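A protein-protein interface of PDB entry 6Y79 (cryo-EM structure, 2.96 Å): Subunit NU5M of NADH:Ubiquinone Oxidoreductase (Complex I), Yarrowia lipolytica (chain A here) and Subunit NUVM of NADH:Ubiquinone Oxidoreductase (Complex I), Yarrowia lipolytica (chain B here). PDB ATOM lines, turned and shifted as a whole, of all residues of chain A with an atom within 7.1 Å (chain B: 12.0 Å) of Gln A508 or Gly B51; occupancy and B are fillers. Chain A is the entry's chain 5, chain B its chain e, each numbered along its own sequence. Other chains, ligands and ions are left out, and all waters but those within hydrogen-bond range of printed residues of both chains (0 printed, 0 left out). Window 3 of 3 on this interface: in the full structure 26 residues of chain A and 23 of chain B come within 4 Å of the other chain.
Ile A506 touches just one residue of chain B: Asn B54. Gln A508 touches two residues of chain B. No residue of chain B comes within 4 Å of Phe A509. Tyr A510 touches none of the printed residues of chain B. Printed residues of chain B within 4 Å of Lys A511: Ala B48 and Met B49. Glu B45 touches none of the printed residues of chain A. Of the printed residues of chain A, Leu B50 touches Gln A508 (3.5 Å) and Leu A512 (3.9 Å). Gly B51 touches one residue of chain A. Of the printed residues of chain A, Tyr B56 touches Ser A505 (2.6 Å). The nearest residue of chain B that does not touch Gln A508 is Leu B52 (4.6 Å).
The side-chain amide oxygen of Asn B54 lies close to the backbone NH of Tyr B56, at 3.2 Å.
Hydrophobic or aromatic side chains of chain A within 4 Å of the printed part of chain B: Tyr A393 and Leu A512. Of the 16 printed residues of chain B, 6 touch a printed residue of chain A. Hydrophobic or aromatic side chains of chain B that line the printed part of chain A: Met B49 and Tyr B56. Along chain B the printed residues that touch a printed residue of chain A span positions 48 to 56. Among the printed residues, 8 pairs touch across the chains.
NZ of Lys A511 is in hydrogen-bond range of O of Ala B48, 2.9 Å away. The side-chain sulfur (SD) of Met B49 sits close to the side-chain hydroxyl (OH) of Tyr A393, at 3.4 Å. The backbone carbonyl oxygen of Leu B50 lies within hydrogen-bond range of the side-chain amide nitrogen of Gln A508 (3.5 Å). O of Gly B51 is in hydrogen-bond range of NE2 of Gln A508 (2.9 Å). ND2 of Asn B54 lies within hydrogen-bond range of O of Ile A506 (2.6 Å). O of Ser A505 lies within hydrogen-bond range of OH of Tyr B56 (2.6 Å).
Lys A511 touches Met B49 (CE to O, 3.9999 Å). Leu B50 touches Leu A512 (O to CB, 3.9 Å).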
ATOM      1  N   TYR A 393      27.887  -1.599  18.549  1.00  0.00           N
ATOM      2  CA  TYR A 393      26.606  -1.957  19.148  1.00  0.00           C
ATOM      3  C   TYR A 393      26.110  -3.277  18.575  1.00  0.00           C
ATOM      4  O   TYR A 393      26.053  -4.298  19.275  1.00  0.00           O
ATOM      5  CB  TYR A 393      25.560  -0.854  18.909  1.00  0.00           C
ATOM      6  CG  TYR A 393      24.255  -1.188  19.599  1.00  0.00           C
ATOM      7  CD1 TYR A 393      24.097  -0.938  20.947  1.00  0.00           C
ATOM      8  CD2 TYR A 393      23.214  -1.821  18.925  1.00  0.00           C
ATOM      9  CE1 TYR A 393      22.943  -1.271  21.601  1.00  0.00           C
ATOM     10  CE2 TYR A 393      22.061  -2.179  19.576  1.00  0.00           C
ATOM     11  CZ  TYR A 393      21.934  -1.898  20.913  1.00  0.00           C
ATOM     12  OH  TYR A 393      20.781  -2.234  21.578  1.00  0.00           O
ATOM     13  N   SER A 505      13.882 -13.667  25.471  1.00  0.00           N
ATOM     14  CA  SER A 505      13.872 -14.030  26.880  1.00  0.00           C
ATOM     15  C   SER A 505      14.746 -13.138  27.733  1.00  0.00           C
ATOM     16  O   SER A 505      14.954 -13.458  28.908  1.00  0.00           O
ATOM     17  CB  SER A 505      14.318 -15.481  27.077  1.00  0.00           C
ATOM     18  OG  SER A 505      14.517 -15.746  28.456  1.00  0.00           O
ATOM     19  N   ILE A 506      15.271 -12.047  27.199  1.00  0.00           N
ATOM     20  CA  ILE A 506      16.120 -11.197  28.017  1.00  0.00           C
ATOM     21  C   ILE A 506      15.259 -10.242  28.831  1.00  0.00           C
ATOM     22  O   ILE A 506      14.251  -9.705  28.352  1.00  0.00           O
ATOM     23  CB  ILE A 506      17.177 -10.462  27.171  1.00  0.00           C
ATOM     24  CG1 ILE A 506      18.112  -9.692  28.102  1.00  0.00           C
ATOM     25  CG2 ILE A 506      16.567  -9.552  26.113  1.00  0.00           C
ATOM     26  CD1 ILE A 506      19.406  -9.405  27.580  1.00  0.00           C
ATOM     27  N   THR A 507      15.628 -10.090  30.093  1.00  0.00           N
ATOM     28  CA  THR A 507      15.159  -9.078  31.012  1.00  0.00           C
ATOM     29  C   THR A 507      15.423  -7.677  30.455  1.00  0.00           C
ATOM     30  O   THR A 507      16.328  -7.455  29.645  1.00  0.00           O
ATOM     31  CB  THR A 507      15.881  -9.285  32.342  1.00  0.00           C
ATOM     32  OG1 THR A 507      15.866 -10.688  32.637  1.00  0.00           O
ATOM     33  CG2 THR A 507      15.212  -8.537  33.522  1.00  0.00           C
ATOM     34  N   GLN A 508      14.572  -6.739  30.876  1.00  0.00           N
ATOM     35  CA  GLN A 508      14.817  -5.315  30.688  1.00  0.00           C
ATOM     36  C   GLN A 508      16.142  -4.908  31.306  1.00  0.00           C
ATOM     37  O   GLN A 508      16.893  -4.113  30.740  1.00  0.00           O
ATOM     38  CB  GLN A 508      13.703  -4.548  31.375  1.00  0.00           C
ATOM     39  CG  GLN A 508      13.364  -3.231  30.761  1.00  0.00           C
ATOM     40  CD  GLN A 508      14.279  -2.091  31.193  1.00  0.00           C
ATOM     41  OE1 GLN A 508      14.726  -2.028  32.329  1.00  0.00           O
ATOM     42  NE2 GLN A 508      14.524  -1.176  30.281  1.00  0.00           N
ATOM     43  N   PHE A 509      16.441  -5.472  32.471  1.00  0.00           N
ATOM     44  CA  PHE A 509      17.651  -5.155  33.221  1.00  0.00           C
ATOM     45  C   PHE A 509      18.886  -5.711  32.534  1.00  0.00           C
ATOM     46  O   PHE A 509      19.895  -5.015  32.400  1.00  0.00           O
ATOM     47  CB  PHE A 509      17.493  -5.722  34.629  1.00  0.00           C
ATOM     48  CG  PHE A 509      18.652  -5.502  35.539  1.00  0.00           C
ATOM     49  CD1 PHE A 509      19.054  -4.227  35.897  1.00  0.00           C
ATOM     50  CD2 PHE A 509      19.297  -6.593  36.093  1.00  0.00           C
ATOM     51  CE1 PHE A 509      20.113  -4.044  36.768  1.00  0.00           C
ATOM     52  CE2 PHE A 509      20.347  -6.418  36.967  1.00  0.00           C
ATOM     53  CZ  PHE A 509      20.754  -5.144  37.308  1.00  0.00           C
ATOM     54  N   TYR A 510      18.806  -6.948  32.043  1.00  0.00           N
ATOM     55  CA  TYR A 510      19.977  -7.580  31.443  1.00  0.00           C
ATOM     56  C   TYR A 510      20.313  -6.988  30.078  1.00  0.00           C
ATOM     57  O   TYR A 510      21.470  -7.059  29.651  1.00  0.00           O
ATOM     58  CB  TYR A 510      19.759  -9.087  31.322  1.00  0.00           C
ATOM     59  CG  TYR A 510      19.792  -9.841  32.629  1.00  0.00           C
ATOM     60  CD1 TYR A 510      20.501  -9.357  33.718  1.00  0.00           C
ATOM     61  CD2 TYR A 510      19.101 -11.037  32.774  1.00  0.00           C
ATOM     62  CE1 TYR A 510      20.527 -10.047  34.918  1.00  0.00           C
ATOM     63  CE2 TYR A 510      19.118 -11.730  33.970  1.00  0.00           C
ATOM     64  CZ  TYR A 510      19.834 -11.231  35.034  1.00  0.00           C
ATOM     65  OH  TYR A 510      19.857 -11.914  36.224  1.00  0.00           O
ATOM     66  N   LYS A 511      19.335  -6.410  29.377  1.00  0.00           N
ATOM     67  CA  LYS A 511      19.633  -5.744  28.112  1.00  0.00           C
ATOM     68  C   LYS A 511      20.011  -4.281  28.325  1.00  0.00           C
ATOM     69  O   LYS A 511      20.953  -3.784  27.695  1.00  0.00           O
ATOM     70  CB  LYS A 511      18.448  -5.842  27.152  1.00  0.00           C
ATOM     71  CG  LYS A 511      18.788  -5.298  25.778  1.00  0.00           C
ATOM     72  CD  LYS A 511      17.687  -5.474  24.770  1.00  0.00           C
ATOM     73  CE  LYS A 511      18.221  -5.128  23.396  1.00  0.00           C
ATOM     74  NZ  LYS A 511      17.291  -5.515  22.302  1.00  0.00           N
ATOM     75  N   LEU A 512      19.271  -3.572  29.201  1.00  0.00           N
ATOM     76  CA  LEU A 512      19.618  -2.214  29.645  1.00  0.00           C
ATOM     77  C   LEU A 512      21.008  -2.120  30.251  1.00  0.00           C
ATOM     78  O   LEU A 512      21.652  -1.080  30.111  1.00  0.00           O
ATOM     79  CB  LEU A 512      18.573  -1.701  30.665  1.00  0.00           C
ATOM     80  CG  LEU A 512      18.635  -0.409  31.499  1.00  0.00           C
ATOM     81  CD1 LEU A 512      17.247   0.270  31.758  1.00  0.00           C
ATOM     82  CD2 LEU A 512      19.337  -0.616  32.905  1.00  0.00           C
ATOM     83  N   LEU A 513      21.495  -3.201  30.854  1.00  0.00           N
ATOM     84  CA  LEU A 513      22.651  -3.127  31.744  1.00  0.00           C
ATOM     85  C   LEU A 513      23.982  -2.826  31.050  1.00  0.00           C
ATOM     86  O   LEU A 513      24.669  -1.889  31.499  1.00  0.00           O
ATOM     87  CB  LEU A 513      22.686  -4.413  32.578  1.00  0.00           C
ATOM     88  CG  LEU A 513      23.619  -4.790  33.715  1.00  0.00           C
ATOM     89  CD1 LEU A 513      22.865  -5.746  34.551  1.00  0.00           C
ATOM     90  CD2 LEU A 513      24.729  -5.538  33.141  1.00  0.00           C
ATOM     91  N   ARG B  41      19.679   6.881  15.281  1.00  0.00           N
ATOM     92  CA  ARG B  41      19.548   5.466  15.593  1.00  0.00           C
ATOM     93  C   ARG B  41      19.126   5.202  17.035  1.00  0.00           C
ATOM     94  O   ARG B  41      18.598   4.123  17.304  1.00  0.00           O
ATOM     95  CB  ARG B  41      20.852   4.740  15.274  1.00  0.00           C
ATOM     96  CG  ARG B  41      21.179   4.681  13.787  1.00  0.00           C
ATOM     97  CD  ARG B  41      20.279   3.702  13.046  1.00  0.00           C
ATOM     98  NE  ARG B  41      19.229   4.366  12.277  1.00  0.00           N
ATOM     99  CZ  ARG B  41      18.112   3.770  11.875  1.00  0.00           C
ATOM    100  NH1 ARG B  41      17.206   4.441  11.180  1.00  0.00           N
ATOM    101  NH2 ARG B  41      17.894   2.499  12.180  1.00  0.00           N
ATOM    102  N   ILE B  42      19.339   6.143  17.966  1.00  0.00           N
ATOM    103  CA  ILE B  42      18.632   6.071  19.249  1.00  0.00           C
ATOM    104  C   ILE B  42      17.153   6.351  19.036  1.00  0.00           C
ATOM    105  O   ILE B  42      16.289   5.679  19.619  1.00  0.00           O
ATOM    106  CB  ILE B  42      19.204   7.053  20.296  1.00  0.00           C
ATOM    107  CG1 ILE B  42      20.676   6.817  20.611  1.00  0.00           C
ATOM    108  CG2 ILE B  42      18.455   6.928  21.621  1.00  0.00           C
ATOM    109  CD1 ILE B  42      20.971   5.498  21.128  1.00  0.00           C
ATOM    110  N   LYS B  43      16.850   7.347  18.190  1.00  0.00           N
ATOM    111  CA  LYS B  43      15.483   7.787  17.962  1.00  0.00           C
ATOM    112  C   LYS B  43      14.619   6.666  17.390  1.00  0.00           C
ATOM    113  O   LYS B  43      13.543   6.381  17.916  1.00  0.00           O
ATOM    114  CB  LYS B  43      15.493   8.990  17.024  1.00  0.00           C
ATOM    115  CG  LYS B  43      14.122   9.430  16.567  1.00  0.00           C
ATOM    116  CD  LYS B  43      14.163   9.750  15.075  1.00  0.00           C
ATOM    117  CE  LYS B  43      12.779   9.997  14.509  1.00  0.00           C
ATOM    118  NZ  LYS B  43      12.458  11.451  14.490  1.00  0.00           N
ATOM    119  N   GLU B  44      15.080   5.986  16.348  1.00  0.00           N
ATOM    120  CA  GLU B  44      14.222   4.986  15.720  1.00  0.00           C
ATOM    121  C   GLU B  44      14.258   3.641  16.448  1.00  0.00           C
ATOM    122  O   GLU B  44      13.259   2.930  16.444  1.00  0.00           O
ATOM    123  CB  GLU B  44      14.621   4.878  14.238  1.00  0.00           C
ATOM    124  CG  GLU B  44      14.006   3.803  13.348  1.00  0.00           C
ATOM    125  CD  GLU B  44      12.525   3.530  13.519  1.00  0.00           C
ATOM    126  OE1 GLU B  44      12.188   2.329  13.507  1.00  0.00           O
ATOM    127  OE2 GLU B  44      11.700   4.466  13.608  1.00  0.00           O
ATOM    128  N   GLU B  45      15.336   3.300  17.143  1.00  0.00           N
ATOM    129  CA  GLU B  45      15.451   1.969  17.729  1.00  0.00           C
ATOM    130  C   GLU B  45      15.115   1.976  19.225  1.00  0.00           C
ATOM    131  O   GLU B  45      15.266   0.949  19.878  1.00  0.00           O
ATOM    132  CB  GLU B  45      16.847   1.387  17.468  1.00  0.00           C
ATOM    133  CG  GLU B  45      16.902  -0.134  17.408  1.00  0.00           C
ATOM    134  CD  GLU B  45      18.319  -0.685  17.411  1.00  0.00           C
ATOM    135  OE1 GLU B  45      19.268   0.091  17.154  1.00  0.00           O
ATOM    136  OE2 GLU B  45      18.476  -1.871  17.772  1.00  0.00           O
ATOM    137  N   TYR B  46      14.561   3.100  19.739  1.00  0.00           N
ATOM    138  CA  TYR B  46      14.371   3.342  21.178  1.00  0.00           C
ATOM    139  C   TYR B  46      13.711   2.199  21.968  1.00  0.00           C
ATOM    140  O   TYR B  46      14.334   1.734  22.947  1.00  0.00           O
ATOM    141  CB  TYR B  46      13.620   4.677  21.365  1.00  0.00           C
ATOM    142  CG  TYR B  46      13.400   5.111  22.797  1.00  0.00           C
ATOM    143  CD1 TYR B  46      14.386   5.805  23.489  1.00  0.00           C
ATOM    144  CD2 TYR B  46      12.198   4.843  23.453  1.00  0.00           C
ATOM    145  CE1 TYR B  46      14.191   6.215  24.794  1.00  0.00           C
ATOM    146  CE2 TYR B  46      11.998   5.241  24.766  1.00  0.00           C
ATOM    147  CZ  TYR B  46      13.000   5.922  25.429  1.00  0.00           C
ATOM    148  OH  TYR B  46      12.804   6.327  26.727  1.00  0.00           O
ATOM    149  N   PRO B  47      12.533   1.649  21.589  1.00  0.00           N
ATOM    150  CA  PRO B  47      11.976   0.562  22.415  1.00  0.00           C
ATOM    151  C   PRO B  47      12.721  -0.755  22.269  1.00  0.00           C
ATOM    152  O   PRO B  47      12.670  -1.584  23.185  1.00  0.00           O
ATOM    153  CB  PRO B  47      10.532   0.449  21.915  1.00  0.00           C
ATOM    154  CG  PRO B  47      10.632   0.784  20.494  1.00  0.00           C
ATOM    155  CD  PRO B  47      11.642   1.896  20.426  1.00  0.00           C
ATOM    156  N   ALA B  48      13.410  -0.977  21.150  1.00  0.00           N
ATOM    157  CA  ALA B  48      14.254  -2.159  21.023  1.00  0.00           C
ATOM    158  C   ALA B  48      15.598  -1.939  21.704  1.00  0.00           C
ATOM    159  O   ALA B  48      16.129  -2.847  22.350  1.00  0.00           O
ATOM    160  CB  ALA B  48      14.446  -2.511  19.549  1.00  0.00           C
ATOM    161  N   MET B  49      16.156  -0.729  21.554  1.00  0.00           N
ATOM    162  CA  MET B  49      17.457  -0.357  22.119  1.00  0.00           C
ATOM    163  C   MET B  49      17.491  -0.507  23.624  1.00  0.00           C
ATOM    164  O   MET B  49      18.354  -1.206  24.170  1.00  0.00           O
ATOM    165  CB  MET B  49      17.778   1.096  21.779  1.00  0.00           C
ATOM    166  CG  MET B  49      19.168   1.537  22.101  1.00  0.00           C
ATOM    167  SD  MET B  49      20.207   0.969  20.768  1.00  0.00           S
ATOM    168  CE  MET B  49      20.036   2.284  19.558  1.00  0.00           C
ATOM    169  N   LEU B  50      16.587   0.188  24.315  1.00  0.00           N
ATOM    170  CA  LEU B  50      16.643   0.152  25.768  1.00  0.00           C
ATOM    171  C   LEU B  50      16.091  -1.155  26.309  1.00  0.00           C
ATOM    172  O   LEU B  50      16.444  -1.570  27.420  1.00  0.00           O
ATOM    173  CB  LEU B  50      15.868   1.321  26.364  1.00  0.00           C
ATOM    174  CG  LEU B  50      16.285   2.749  26.044  1.00  0.00           C
ATOM    175  CD1 LEU B  50      15.457   3.660  26.903  1.00  0.00           C
ATOM    176  CD2 LEU B  50      17.751   2.968  26.310  1.00  0.00           C
ATOM    177  N   GLY B  51      15.220  -1.799  25.540  1.00  0.00           N
ATOM    178  CA  GLY B  51      14.517  -2.976  25.993  1.00  0.00           C
ATOM    179  C   GLY B  51      13.246  -2.519  26.677  1.00  0.00           C
ATOM    180  O   GLY B  51      13.299  -2.020  27.803  1.00  0.00           O
ATOM    181  N   LEU B  52      12.119  -2.597  25.978  1.00  0.00           N
ATOM    182  CA  LEU B  52      10.809  -2.316  26.556  1.00  0.00           C
ATOM    183  C   LEU B  52       9.794  -3.218  25.868  1.00  0.00           C
ATOM    184  O   LEU B  52      10.134  -3.916  24.914  1.00  0.00           O
ATOM    185  CB  LEU B  52      10.376  -0.835  26.441  1.00  0.00           C
ATOM    186  CG  LEU B  52      10.874   0.274  27.383  1.00  0.00           C
ATOM    187  CD1 LEU B  52      12.170   0.928  26.928  1.00  0.00           C
ATOM    188  CD2 LEU B  52       9.736   1.270  27.623  1.00  0.00           C
ATOM    189  N   HIS B  53       8.551  -3.184  26.364  1.00  0.00           N
ATOM    190  CA  HIS B  53       7.409  -4.040  25.980  1.00  0.00           C
ATOM    191  C   HIS B  53       7.811  -5.516  25.813  1.00  0.00           C
ATOM    192  O   HIS B  53       7.635  -6.130  24.761  1.00  0.00           O
ATOM    193  CB  HIS B  53       6.675  -3.487  24.737  1.00  0.00           C
ATOM    194  CG  HIS B  53       7.474  -3.468  23.459  1.00  0.00           C
ATOM    195  ND1 HIS B  53       8.364  -2.465  23.141  1.00  0.00           N
ATOM    196  CD2 HIS B  53       7.469  -4.310  22.396  1.00  0.00           C
ATOM    197  CE1 HIS B  53       8.897  -2.709  21.957  1.00  0.00           C
ATOM    198  NE2 HIS B  53       8.376  -3.826  21.485  1.00  0.00           N
ATOM    199  N   ASN B  54       8.346  -6.092  26.891  1.00  0.00           N
ATOM    200  CA  ASN B  54       8.875  -7.447  26.759  1.00  0.00           C
ATOM    201  C   ASN B  54       7.752  -8.469  26.599  1.00  0.00           C
ATOM    202  O   ASN B  54       6.640  -8.310  27.108  1.00  0.00           O
ATOM    203  CB  ASN B  54       9.760  -7.850  27.942  1.00  0.00           C
ATOM    204  CG  ASN B  54      10.623  -9.081  27.637  1.00  0.00           C
ATOM    205  OD1 ASN B  54      10.121 -10.203  27.517  1.00  0.00           O
ATOM    206  ND2 ASN B  54      11.928  -8.859  27.484  1.00  0.00           N
ATOM    207  N   PHE B  55       8.096  -9.536  25.885  1.00  0.00           N
ATOM    208  CA  PHE B  55       7.198 -10.491  25.267  1.00  0.00           C
ATOM    209  C   PHE B  55       6.852 -11.669  26.176  1.00  0.00           C
ATOM    210  O   PHE B  55       6.257 -12.645  25.700  1.00  0.00           O
ATOM    211  CB  PHE B  55       7.850 -10.967  23.963  1.00  0.00           C
ATOM    212  CG  PHE B  55       8.205  -9.832  23.030  1.00  0.00           C
ATOM    213  CD1 PHE B  55       7.275  -8.837  22.768  1.00  0.00           C
ATOM    214  CD2 PHE B  55       9.473  -9.723  22.465  1.00  0.00           C
ATOM    215  CE1 PHE B  55       7.578  -7.776  21.931  1.00  0.00           C
ATOM    216  CE2 PHE B  55       9.787  -8.657  21.622  1.00  0.00           C
ATOM    217  CZ  PHE B  55       8.834  -7.682  21.359  1.00  0.00           C
ATOM    218  N   TYR B  56       7.230 -11.614  27.457  1.00  0.00           N
ATOM    219  CA  TYR B  56       6.658 -12.523  28.446  1.00  0.00           C
ATOM    220  C   TYR B  56       5.174 -12.217  28.609  1.00  0.00           C
ATOM    221  O   TYR B  56       4.793 -11.041  28.656  1.00  0.00           O
ATOM    222  CB  TYR B  56       7.341 -12.397  29.809  1.00  0.00           C
ATOM    223  CG  TYR B  56       8.777 -12.861  29.853  1.00  0.00           C
ATOM    224  CD1 TYR B  56       9.085 -14.190  29.714  1.00  0.00           C
ATOM    225  CD2 TYR B  56       9.814 -11.969  30.092  1.00  0.00           C
ATOM    226  CE1 TYR B  56      10.380 -14.635  29.755  1.00  0.00           C
ATOM    227  CE2 TYR B  56      11.131 -12.399  30.148  1.00  0.00           C
ATOM    228  CZ  TYR B  56      11.406 -13.738  29.975  1.00  0.00           C
ATOM    229  OH  TYR B  56      12.710 -14.166  30.027  1.00  0.00           O
